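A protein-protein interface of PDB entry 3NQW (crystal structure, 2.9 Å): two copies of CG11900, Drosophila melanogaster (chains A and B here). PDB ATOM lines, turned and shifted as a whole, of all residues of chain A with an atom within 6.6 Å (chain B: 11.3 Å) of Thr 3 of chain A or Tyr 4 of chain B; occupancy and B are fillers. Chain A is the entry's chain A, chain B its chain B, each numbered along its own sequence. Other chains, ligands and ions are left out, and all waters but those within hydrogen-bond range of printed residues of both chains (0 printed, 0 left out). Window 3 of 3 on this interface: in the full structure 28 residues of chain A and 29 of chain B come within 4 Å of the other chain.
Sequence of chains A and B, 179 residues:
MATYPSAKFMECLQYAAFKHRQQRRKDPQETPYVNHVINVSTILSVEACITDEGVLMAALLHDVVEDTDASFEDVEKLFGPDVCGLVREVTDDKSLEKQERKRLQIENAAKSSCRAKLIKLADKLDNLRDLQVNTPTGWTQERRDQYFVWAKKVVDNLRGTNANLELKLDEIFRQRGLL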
ATOM      1  N   ALA A   2       6.912  21.483   6.481  1.00  0.00           N
ATOM      2  CA  ALA A   2       7.391  22.257   7.661  1.00  0.00           C
ATOM      3  C   ALA A   2       6.569  23.535   7.851  1.00  0.00           C
ATOM      4  O   ALA A   2       6.770  24.270   8.816  1.00  0.00           O
ATOM      5  CB  ALA A   2       8.878  22.602   7.489  1.00  0.00           C
ATOM      6  N   THR A   3       5.638  23.797   6.937  1.00  0.00           N
ATOM      7  CA  THR A   3       4.805  24.991   7.031  1.00  0.00           C
ATOM      8  C   THR A   3       3.327  24.669   7.228  1.00  0.00           C
ATOM      9  O   THR A   3       2.877  23.550   6.976  1.00  0.00           O
ATOM     10  CB  THR A   3       4.921  25.858   5.775  1.00  0.00           C
ATOM     11  OG1 THR A   3       4.124  25.297   4.724  1.00  0.00           O
ATOM     12  CG2 THR A   3       6.360  25.922   5.320  1.00  0.00           C
ATOM     13  N   TYR A   4       2.575  25.677   7.663  1.00  0.00           N
ATOM     14  CA  TYR A   4       1.144  25.541   7.912  1.00  0.00           C
ATOM     15  C   TYR A   4       0.552  26.912   8.120  1.00  0.00           C
ATOM     16  O   TYR A   4       1.215  27.814   8.640  1.00  0.00           O
ATOM     17  CB  TYR A   4       0.888  24.715   9.166  1.00  0.00           C
ATOM     18  CG  TYR A   4       1.486  25.316  10.415  1.00  0.00           C
ATOM     19  CD1 TYR A   4       2.870  25.293  10.624  1.00  0.00           C
ATOM     20  CD2 TYR A   4       0.678  25.943  11.371  1.00  0.00           C
ATOM     21  CE1 TYR A   4       3.442  25.879  11.749  1.00  0.00           C
ATOM     22  CE2 TYR A   4       1.235  26.535  12.503  1.00  0.00           C
ATOM     23  CZ  TYR A   4       2.621  26.501  12.689  1.00  0.00           C
ATOM     24  OH  TYR A   4       3.194  27.082  13.804  1.00  0.00           O
ATOM     25  N   PRO A   5      -0.710  27.090   7.723  1.00  0.00           N
ATOM     26  CA  PRO A   5      -1.389  28.374   7.875  1.00  0.00           C
ATOM     27  C   PRO A   5      -1.743  28.585   9.331  1.00  0.00           C
ATOM     28  O   PRO A   5      -2.129  27.648  10.033  1.00  0.00           O
ATOM     29  CB  PRO A   5      -2.621  28.222   6.992  1.00  0.00           C
ATOM     30  CG  PRO A   5      -2.936  26.775   7.126  1.00  0.00           C
ATOM     31  CD  PRO A   5      -1.572  26.125   7.025  1.00  0.00           C
ATOM     32  N   SER A   6      -1.582  29.825   9.773  1.00  0.00           N
ATOM     33  CA  SER A   6      -1.860  30.246  11.139  1.00  0.00           C
ATOM     34  C   SER A   6      -3.352  30.184  11.438  1.00  0.00           C
ATOM     35  O   SER A   6      -4.164  29.994  10.530  1.00  0.00           O
ATOM     36  CB  SER A   6      -1.379  31.687  11.326  1.00  0.00           C
ATOM     37  OG  SER A   6      -2.141  32.595  10.523  1.00  0.00           O
ATOM     38  N   SER A  45       0.036  32.300  -4.153  1.00  0.00           N
ATOM     39  CA  SER A  45       0.736  31.224  -3.493  1.00  0.00           C
ATOM     40  C   SER A  45       1.386  30.252  -4.469  1.00  0.00           C
ATOM     41  O   SER A  45       2.603  30.081  -4.440  1.00  0.00           O
ATOM     42  CB  SER A  45      -0.199  30.480  -2.560  1.00  0.00           C
ATOM     43  OG  SER A  45       0.567  29.791  -1.587  1.00  0.00           O
ATOM     44  N   ILE A  50       4.220  33.137  -3.243  1.00  0.00           N
ATOM     45  CA  ILE A  50       4.286  34.049  -2.089  1.00  0.00           C
ATOM     46  C   ILE A  50       4.217  33.341  -0.719  1.00  0.00           C
ATOM     47  O   ILE A  50       3.257  32.635  -0.403  1.00  0.00           O
ATOM     48  CB  ILE A  50       3.201  35.187  -2.163  1.00  0.00           C
ATOM     49  CG1 ILE A  50       3.667  36.318  -3.094  1.00  0.00           C
ATOM     50  CG2 ILE A  50       3.009  35.824  -0.789  1.00  0.00           C
ATOM     51  CD1 ILE A  50       3.606  36.017  -4.578  1.00  0.00           C
ATOM     52  N   THR A  51       5.252  33.566   0.089  1.00  0.00           N
ATOM     53  CA  THR A  51       5.412  32.956   1.409  1.00  0.00           C
ATOM     54  C   THR A  51       5.045  33.862   2.612  1.00  0.00           C
ATOM     55  O   THR A  51       5.424  33.584   3.761  1.00  0.00           O
ATOM     56  CB  THR A  51       6.886  32.411   1.532  1.00  0.00           C
ATOM     57  OG1 THR A  51       7.840  33.453   1.283  1.00  0.00           O
ATOM     58  CG2 THR A  51       7.117  31.306   0.501  1.00  0.00           C
ATOM     59  N   ASP A  52       4.279  34.921   2.328  1.00  0.00           N
ATOM     60  CA  ASP A  52       3.845  35.928   3.312  1.00  0.00           C
ATOM     61  C   ASP A  52       2.337  35.987   3.539  1.00  0.00           C
ATOM     62  O   ASP A  52       1.586  36.504   2.707  1.00  0.00           O
ATOM     63  CB  ASP A  52       4.326  37.316   2.867  1.00  0.00           C
ATOM     64  CG  ASP A  52       4.043  38.389   3.891  1.00  0.00           C
ATOM     65  OD1 ASP A  52       2.881  38.820   4.007  1.00  0.00           O
ATOM     66  OD2 ASP A  52       4.988  38.802   4.598  1.00  0.00           O
ATOM     67  N   GLU A  53       1.908  35.461   4.681  1.00  0.00           N
ATOM     68  CA  GLU A  53       0.495  35.454   5.057  1.00  0.00           C
ATOM     69  C   GLU A  53      -0.183  36.832   5.002  1.00  0.00           C
ATOM     70  O   GLU A  53      -1.357  36.940   4.636  1.00  0.00           O
ATOM     71  CB  GLU A  53       0.329  34.864   6.458  1.00  0.00           C
ATOM     72  CG  GLU A  53      -0.089  33.414   6.449  1.00  0.00           C
ATOM     73  CD  GLU A  53      -0.266  32.850   7.836  1.00  0.00           C
ATOM     74  OE1 GLU A  53      -0.774  31.714   7.949  1.00  0.00           O
ATOM     75  OE2 GLU A  53       0.109  33.535   8.817  1.00  0.00           O
ATOM     76  N   LEU A  56      -1.353  37.046   1.636  1.00  0.00           N
ATOM     77  CA  LEU A  56      -2.327  35.982   1.420  1.00  0.00           C
ATOM     78  C   LEU A  56      -3.693  36.324   2.023  1.00  0.00           C
ATOM     79  O   LEU A  56      -4.712  36.267   1.342  1.00  0.00           O
ATOM     80  CB  LEU A  56      -1.798  34.671   2.011  1.00  0.00           C
ATOM     81  CG  LEU A  56      -0.497  34.156   1.387  1.00  0.00           C
ATOM     82  CD1 LEU A  56      -0.016  32.929   2.146  1.00  0.00           C
ATOM     83  CD2 LEU A  56      -0.718  33.834  -0.090  1.00  0.00           C
ATOM     84  N   ALA B   2       6.369  33.505  12.526  1.00  0.00           N
ATOM     85  CA  ALA B   2       6.528  33.615  11.081  1.00  0.00           C
ATOM     86  C   ALA B   2       5.989  32.370  10.358  1.00  0.00           C
ATOM     87  O   ALA B   2       6.762  31.510   9.929  1.00  0.00           O
ATOM     88  CB  ALA B   2       8.001  33.823  10.753  1.00  0.00           C
ATOM     89  N   THR B   3       4.665  32.289  10.222  1.00  0.00           N
ATOM     90  CA  THR B   3       3.989  31.152   9.578  1.00  0.00           C
ATOM     91  C   THR B   3       3.322  31.504   8.248  1.00  0.00           C
ATOM     92  O   THR B   3       3.162  32.682   7.922  1.00  0.00           O
ATOM     93  CB  THR B   3       2.896  30.577  10.485  1.00  0.00           C
ATOM     94  OG1 THR B   3       1.782  31.474  10.501  1.00  0.00           O
ATOM     95  CG2 THR B   3       3.408  30.413  11.901  1.00  0.00           C
ATOM     96  N   TYR B   4       2.911  30.480   7.493  1.00  0.00           N
ATOM     97  CA  TYR B   4       2.266  30.694   6.192  1.00  0.00           C
ATOM     98  C   TYR B   4       1.884  29.400   5.486  1.00  0.00           C
ATOM     99  O   TYR B   4       2.667  28.460   5.436  1.00  0.00           O
ATOM    100  CB  TYR B   4       3.194  31.461   5.266  1.00  0.00           C
ATOM    101  CG  TYR B   4       4.425  30.679   4.876  1.00  0.00           C
ATOM    102  CD1 TYR B   4       5.525  30.587   5.741  1.00  0.00           C
ATOM    103  CD2 TYR B   4       4.497  30.026   3.638  1.00  0.00           C
ATOM    104  CE1 TYR B   4       6.669  29.871   5.377  1.00  0.00           C
ATOM    105  CE2 TYR B   4       5.629  29.306   3.262  1.00  0.00           C
ATOM    106  CZ  TYR B   4       6.714  29.237   4.130  1.00  0.00           C
ATOM    107  OH  TYR B   4       7.861  28.584   3.735  1.00  0.00           O
ATOM    108  N   PRO B   5       0.685  29.347   4.892  1.00  0.00           N
ATOM    109  CA  PRO B   5       0.276  28.124   4.202  1.00  0.00           C
ATOM    110  C   PRO B   5       1.156  27.906   3.001  1.00  0.00           C
ATOM    111  O   PRO B   5       1.731  28.850   2.465  1.00  0.00           O
ATOM    112  CB  PRO B   5      -1.164  28.412   3.807  1.00  0.00           C
ATOM    113  CG  PRO B   5      -1.132  29.868   3.535  1.00  0.00           C
ATOM    114  CD  PRO B   5      -0.329  30.398   4.719  1.00  0.00           C
ATOM    115  N   SER B   6       1.269  26.656   2.589  1.00  0.00           N
ATOM    116  CA  SER B   6       2.086  26.311   1.444  1.00  0.00           C
ATOM    117  C   SER B   6       1.269  26.420   0.144  1.00  0.00           C
ATOM    118  O   SER B   6       0.042  26.636   0.173  1.00  0.00           O
ATOM    119  CB  SER B   6       2.616  24.886   1.623  1.00  0.00           C
ATOM    120  OG  SER B   6       1.566  23.930   1.562  1.00  0.00           O
ATOM    121  N   ALA B   7       1.960  26.262  -0.988  1.00  0.00           N
ATOM    122  CA  ALA B   7       1.337  26.319  -2.314  1.00  0.00           C
ATOM    123  C   ALA B   7       0.431  25.111  -2.486  1.00  0.00           C
ATOM    124  O   ALA B   7      -0.582  25.174  -3.180  1.00  0.00           O
ATOM    125  CB  ALA B   7       2.398  26.341  -3.389  1.00  0.00           C
ATOM    126  N   LYS B   8       0.788  24.015  -1.827  1.00  0.00           N
ATOM    127  CA  LYS B   8      -0.016  22.805  -1.891  1.00  0.00           C
ATOM    128  C   LYS B   8      -1.345  23.010  -1.166  1.00  0.00           C
ATOM    129  O   LYS B   8      -2.383  22.528  -1.620  1.00  0.00           O
ATOM    130  CB  LYS B   8       0.733  21.637  -1.246  1.00  0.00           C
ATOM    131  CG  LYS B   8       1.940  21.129  -2.025  1.00  0.00           C
ATOM    132  CD  LYS B   8       1.570  20.145  -3.147  1.00  0.00           C
ATOM    133  CE  LYS B   8       0.951  20.805  -4.354  1.00  0.00           C
ATOM    134  NZ  LYS B   8       0.695  19.758  -5.376  1.00  0.00           N
ATOM    135  N   PHE B   9      -1.309  23.720  -0.039  1.00  0.00           N
ATOM    136  CA  PHE B   9      -2.519  23.973   0.744  1.00  0.00           C
ATOM    137  C   PHE B   9      -3.514  24.921   0.051  1.00  0.00           C
ATOM    138  O   PHE B   9      -4.734  24.841   0.239  1.00  0.00           O
ATOM    139  CB  PHE B   9      -2.147  24.534   2.108  1.00  0.00           C
ATOM    140  CG  PHE B   9      -3.327  24.784   2.983  1.00  0.00           C
ATOM    141  CD1 PHE B   9      -4.024  25.993   2.918  1.00  0.00           C
ATOM    142  CD2 PHE B   9      -3.755  23.807   3.865  1.00  0.00           C
ATOM    143  CE1 PHE B   9      -5.139  26.224   3.732  1.00  0.00           C
ATOM    144  CE2 PHE B   9      -4.860  24.015   4.682  1.00  0.00           C
ATOM    145  CZ  PHE B   9      -5.557  25.228   4.619  1.00  0.00           C
ATOM    146  N   MET B  10      -2.970  25.821  -0.752  1.00  0.00           N
ATOM    147  CA  MET B  10      -3.788  26.761  -1.470  1.00  0.00           C
ATOM    148  C   MET B  10      -4.351  26.045  -2.692  1.00  0.00           C
ATOM    149  O   MET B  10      -5.494  26.285  -3.089  1.00  0.00           O
ATOM    150  CB  MET B  10      -2.949  27.974  -1.855  1.00  0.00           C
ATOM    151  CG  MET B  10      -2.319  28.696  -0.651  1.00  0.00           C
ATOM    152  SD  MET B  10      -3.529  29.181   0.598  1.00  0.00           S
ATOM    153  CE  MET B  10      -4.324  30.526  -0.195  1.00  0.00           C
ATOM    154  N   GLU B  11      -3.554  25.154  -3.285  1.00  0.00           N
ATOM    155  CA  GLU B  11      -4.005  24.380  -4.438  1.00  0.00           C
ATOM    156  C   GLU B  11      -5.082  23.394  -3.971  1.00  0.00           C
ATOM    157  O   GLU B  11      -5.908  22.943  -4.767  1.00  0.00           O
ATOM    158  CB  GLU B  11      -2.827  23.636  -5.073  1.00  0.00           C
ATOM    159  CG  GLU B  11      -3.240  22.577  -6.087  1.00  0.00           C
ATOM    160  CD  GLU B  11      -2.058  21.961  -6.818  1.00  0.00           C
ATOM    161  OE1 GLU B  11      -1.335  22.723  -7.497  1.00  0.00           O
ATOM    162  OE2 GLU B  11      -1.851  20.728  -6.716  1.00  0.00           O
ATOM    163  N   SER B  45      -7.914  24.466  13.026  1.00  0.00           N
ATOM    164  CA  SER B  45      -6.849  25.447  13.123  1.00  0.00           C
ATOM    165  C   SER B  45      -7.004  26.353  14.317  1.00  0.00           C
ATOM    166  O   SER B  45      -6.162  26.375  15.209  1.00  0.00           O
ATOM    167  CB  SER B  45      -6.807  26.338  11.902  1.00  0.00           C
ATOM    168  OG  SER B  45      -5.850  27.347  12.122  1.00  0.00           O
ATOM    169  N   ILE B  50      -4.639  23.277  15.599  1.00  0.00           N
ATOM    170  CA  ILE B  50      -3.878  22.298  14.791  1.00  0.00           C
ATOM    171  C   ILE B  50      -2.845  22.934  13.861  1.00  0.00           C
ATOM    172  O   ILE B  50      -3.174  23.781  13.041  1.00  0.00           O
ATOM    173  CB  ILE B  50      -4.791  21.412  13.904  1.00  0.00           C
ATOM    174  CG1 ILE B  50      -5.844  20.710  14.764  1.00  0.00           C
ATOM    175  CG2 ILE B  50      -3.939  20.365  13.158  1.00  0.00           C
ATOM    176  CD1 ILE B  50      -5.277  19.824  15.859  1.00  0.00           C
ATOM    177  N   THR B  51      -1.600  22.478  13.959  1.00  0.00           N
ATOM    178  CA  THR B  51      -0.505  23.038  13.166  1.00  0.00           C
ATOM    179  C   THR B  51       0.055  22.167  12.019  1.00  0.00           C
ATOM    180  O   THR B  51       1.087  22.492  11.432  1.00  0.00           O
ATOM    181  CB  THR B  51       0.622  23.451  14.141  1.00  0.00           C
ATOM    182  OG1 THR B  51       1.087  22.310  14.881  1.00  0.00           O
ATOM    183  CG2 THR B  51       0.075  24.468  15.128  1.00  0.00           C
ATOM    184  N   ASP B  52      -0.661  21.083  11.705  1.00  0.00           N
ATOM    185  CA  ASP B  52      -0.310  20.111  10.664  1.00  0.00           C
ATOM    186  C   ASP B  52      -1.199  20.235   9.426  1.00  0.00           C
ATOM    187  O   ASP B  52      -2.402  19.957   9.484  1.00  0.00           O
ATOM    188  CB  ASP B  52      -0.458  18.699  11.218  1.00  0.00           C
ATOM    189  CG  ASP B  52      -0.236  17.642  10.173  1.00  0.00           C
ATOM    190  OD1 ASP B  52       0.867  17.594   9.603  1.00  0.00           O
ATOM    191  OD2 ASP B  52      -1.159  16.851   9.922  1.00  0.00           O
ATOM    192  N   GLU B  53      -0.605  20.630   8.305  1.00  0.00           N
ATOM    193  CA  GLU B  53      -1.357  20.781   7.062  1.00  0.00           C
ATOM    194  C   GLU B  53      -2.017  19.509   6.535  1.00  0.00           C
ATOM    195  O   GLU B  53      -3.094  19.572   5.942  1.00  0.00           O
ATOM    196  CB  GLU B  53      -0.472  21.379   5.977  1.00  0.00           C
ATOM    197  CG  GLU B  53      -0.395  22.882   6.056  1.00  0.00           C
ATOM    198  CD  GLU B  53       0.048  23.518   4.753  1.00  0.00           C
ATOM    199  OE1 GLU B  53      -0.055  24.764   4.643  1.00  0.00           O
ATOM    200  OE2 GLU B  53       0.500  22.776   3.844  1.00  0.00           O
ATOM    201  N   GLY B  54      -1.378  18.361   6.740  1.00  0.00           N
ATOM    202  CA  GLY B  54      -1.969  17.124   6.274  1.00  0.00           C
ATOM    203  C   GLY B  54      -3.390  16.938   6.785  1.00  0.00           C
ATOM    204  O   GLY B  54      -4.175  16.209   6.181  1.00  0.00           O
ATOM    205  N   VAL B  55      -3.715  17.593   7.903  1.00  0.00           N
ATOM    206  CA  VAL B  55      -5.044  17.519   8.531  1.00  0.00           C
ATOM    207  C   VAL B  55      -5.921  18.676   8.040  1.00  0.00           C
ATOM    208  O   VAL B  55      -7.121  18.514   7.793  1.00  0.00           O
ATOM    209  CB  VAL B  55      -4.937  17.610  10.085  1.00  0.00           C
ATOM    210  CG1 VAL B  55      -6.324  17.568  10.735  1.00  0.00           C
ATOM    211  CG2 VAL B  55      -4.090  16.469  10.607  1.00  0.00           C
ATOM    212  N   LEU B  56      -5.304  19.845   7.908  1.00  0.00           N
ATOM    213  CA  LEU B  56      -6.005  21.028   7.452  1.00  0.00           C
ATOM    214  C   LEU B  56      -6.425  20.844   5.989  1.00  0.00           C
ATOM    215  O   LEU B  56      -7.507  21.266   5.577  1.00  0.00           O
ATOM    216  CB  LEU B  56      -5.115  22.268   7.642  1.00  0.00           C
ATOM    217  CG  LEU B  56      -4.639  22.520   9.081  1.00  0.00           C
ATOM    218  CD1 LEU B  56      -3.604  23.628   9.096  1.00  0.00           C
ATOM    219  CD2 LEU B  56      -5.825  22.861   9.968  1.00  0.00           C
ATOM    220  N   MET B  57      -5.594  20.196   5.191  1.00  0.00           N
ATOM    221  CA  MET B  57      -5.983  19.983   3.806  1.00  0.00           C
ATOM    222  C   MET B  57      -6.951  18.808   3.767  1.00  0.00           C
ATOM    223  O   MET B  57      -7.891  18.807   2.987  1.00  0.00           O
ATOM    224  CB  MET B  57      -4.762  19.683   2.947  1.00  0.00           C
ATOM    225  CG  MET B  57      -3.751  20.812   2.883  1.00  0.00           C
ATOM    226  SD  MET B  57      -2.149  20.212   2.338  1.00  0.00           S
ATOM    227  CE  MET B  57      -2.558  19.602   0.684  1.00  0.00           C
ATOM    228  N   ASP B  82      -0.367  10.757   1.822  1.00  0.00           N
ATOM    229  CA  ASP B  82      -0.405  11.237   3.202  1.00  0.00           C
ATOM    230  C   ASP B  82      -1.790  11.733   3.569  1.00  0.00           C
ATOM    231  O   ASP B  82      -2.299  11.436   4.653  1.00  0.00           O
ATOM    232  CB  ASP B  82       0.614  12.366   3.372  1.00  0.00           C
ATOM    233  CG  ASP B  82       0.866  13.132   2.068  1.00  0.00           C
ATOM    234  OD1 ASP B  82       1.628  12.625   1.216  1.00  0.00           O
ATOM    235  OD2 ASP B  82       0.292  14.231   1.898  1.00  0.00           O
ATOM    236  N   VAL B  83      -2.379  12.501   2.652  1.00  0.00           N
ATOM    237  CA  VAL B  83      -3.716  13.054   2.813  1.00  0.00           C
ATOM    238  C   VAL B  83      -4.773  12.139   2.165  1.00  0.00           C
ATOM    239  O   VAL B  83      -5.918  12.134   2.598  1.00  0.00           O
ATOM    240  CB  VAL B  83      -3.817  14.477   2.197  1.00  0.00           C
ATOM    241  CG1 VAL B  83      -2.732  15.392   2.769  1.00  0.00           C
ATOM    242  CG2 VAL B  83      -3.693  14.400   0.706  1.00  0.00           C
ATOM    243  N   ARG B 115      -5.604  11.487  13.928  1.00  0.00           N
ATOM    244  CA  ARG B 115      -5.782  12.550  12.931  1.00  0.00           C
ATOM    245  C   ARG B 115      -7.168  12.571  12.273  1.00  0.00           C
ATOM    246  O   ARG B 115      -7.749  13.639  12.071  1.00  0.00           O
ATOM    247  CB  ARG B 115      -4.691  12.447  11.856  1.00  0.00           C
ATOM    248  CG  ARG B 115      -3.275  12.510  12.415  1.00  0.00           C
ATOM    249  CD  ARG B 115      -2.297  13.148  11.413  1.00  0.00           C
ATOM    250  NE  ARG B 115      -1.972  12.271  10.288  1.00  0.00           N
ATOM    251  CZ  ARG B 115      -1.328  12.660   9.189  1.00  0.00           C
ATOM    252  NH1 ARG B 115      -1.074  11.773   8.225  1.00  0.00           N
ATOM    253  NH2 ARG B 115      -0.953  13.930   9.045  1.00  0.00           N
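The side-chain hydroxyl (OG1) of Thr 3 of chain B sits at hydrogen-bond distance from the side-chain carboxylate (OE2) of Glu 53 of chain A (3.1 Å).
The backbone NH of Tyr 4 of chain B lies within hydrogen-bond range of the backbone carbonyl oxygen of Tyr 4 of chain A, at 3.4 Å.
The backbone NH (N) of Ser 6 of chain A sits at hydrogen-bond distance from the side-chain carboxylate (OE1) of Glu 53 of chain A (2.7 Å).
The side-chain hydroxyl (OG) of Ser 6 of chain B lies within hydrogen-bond range of the backbone NH (N) of Phe 9 of chain B, 3.3 Å away.
O of Ser 45 of chain B is in hydrogen-bond range of N of Ile 50 of chain B (3.5 Å).
The side-chain carboxylate of Glu 53 of chain B is in hydrogen-bond range of the side-chain hydroxyl of Ser 6 of chain B (2.8 Å).
OG of Ser 6 of chain B lies close to N of Lys 8 of chain B (3.5 Å).
Among the printed residues, merely in contact across the chains: Tyr 4 of chain A with Thr 51 of chain B (3.0 Å), Pro 5 of chain A with Glu 53 of chain B (3.1 Å), Ser 45 of chain A with Met 10 of chain B (3.2 Å), Thr 51 of chain A with Tyr 4 of chain B (3.3 Å), Ser 6 of chain A with Thr 3 of chain B (3.3 Å), Thr 3 of chain A with Tyr 4 of chain B (3.4 Å), Thr 3 of chain A with Glu 53 of chain B (3.5 Å), Thr 3 of chain A with Ser 6 of chain B (3.5 Å), Glu 53 of chain A with Pro 5 of chain B (3.5 Å), Pro 5 of chain A with Pro 5 of chain B (3.5 Å), Ser 6 of chain A with Ser 45 of chain B (3.5 Å), Leu 56 of chain A with Pro 5 of chain B (3.5 Å), Tyr 4 of chain A with Glu 53 of chain B (3.6 Å), Glu 53 of chain A with Tyr 4 of chain B (3.6 Å), Ser 45 of chain A with Ala 7 of chain B (3.6 Å), Ser 45 of chain A with Ser 6 of chain B (3.7 Å), Tyr 4 of chain A with Thr 3 of chain B (3.7 Å), Pro 5 of chain A with Leu 56 of chain B (3.8 Å) and Pro 5 of chain A with Phe 9 of chain B (3.9 Å).
No residue of chain B comes within 4 Å of Ala 2 of chain A.
Thr 3 of chain A touches just these residues of chain B: Tyr 4, Ser 6 and Glu 53.
Tyr 4 of chain A touches just these residues of chain B: Thr 3, Tyr 4, Thr 51 and Glu 53.
Pro 5 of chain A touches four residues of chain B.
Of the printed residues of chain B, Ser 45 of chain A touches Ser 6, Ala 7 and Met 10.
Ile 50 of chain A touches none of the printed residues of chain B.
Thr 51 of chain A touches one residue of chain B.
Glu 53 of chain A touches just these residues of chain B: Thr 3, Tyr 4 and Pro 5.
Of the printed residues of chain B, Leu 56 of chain A touches Pro 5.
Of the printed residues of chain A, Tyr 4 of chain B touches Thr 3 (3.4 Å), Tyr 4 (3.4 Å), Thr 51 (3.3 Å) and Glu 53 (3.6 Å).
Of the printed residues of chain A, Phe 9 of chain B touches Pro 5.
Ile 50 of chain B touches none of the printed residues of chain A.
Of the printed residues of chain A, Thr 51 of chain B touches Tyr 4 (3.0 Å).
Of the printed residues of chain A, Leu 56 of chain B touches Pro 5.
The nearest residue of chain B that does not touch Thr 3 of chain A is Pro 5 of chain B (4.3 Å).
The nearest printed residue of chain A that does not touch Thr 51 of chain B is Thr 3 of chain A (4.9 Å).
Of the 22 printed residues of chain B, 11 touch a printed residue of chain A.
Printed residues of chain B that touch a printed residue of chain A: Thr 3, Tyr 4, Pro 5, Ser 6, Ala 7, Phe 9, Met 10, Ser 45, Thr 51, Glu 53 and Leu 56.
Hydrophobic or aromatic side chains of chain B that line the printed part of chain A: Tyr 4, Pro 5, Ala 7, Phe 9, Met 10 and Leu 56.
Along chain B the printed residues that touch a printed residue of chain A span positions 3 to 56.
Printed residues of chain A that touch a printed residue of chain B: Thr 3, Tyr 4, Pro 5, Ser 6, Ser 45, Thr 51, Glu 53 and Leu 56.
Hydrophobic or aromatic side chains of chain A within 4 Å of the printed part of chain B: Tyr 4, Pro 5 and Leu 56.
Among the printed residues, 21 pairs touch across the chains.
Thr 3 of chain A touches Ser 6 of chain B, and with the chains exchanged Ser 6 of chain A touches Thr 3 of chain B.
Thr 3 of chain A touches Glu 53 of chain B, and with the chains exchanged Glu 53 of chain A touches Thr 3 of chain B.
Tyr 4 of chain B touches its own counterpart, Tyr 4 of chain A.
Pro 5 of chain A touches Leu 56 of chain B, and with the chains exchanged Leu 56 of chain A touches Pro 5 of chain B.
Of the 21 pairs that touch across the chains among the printed residues, 18 have their exchanged pair printed and touching as well.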
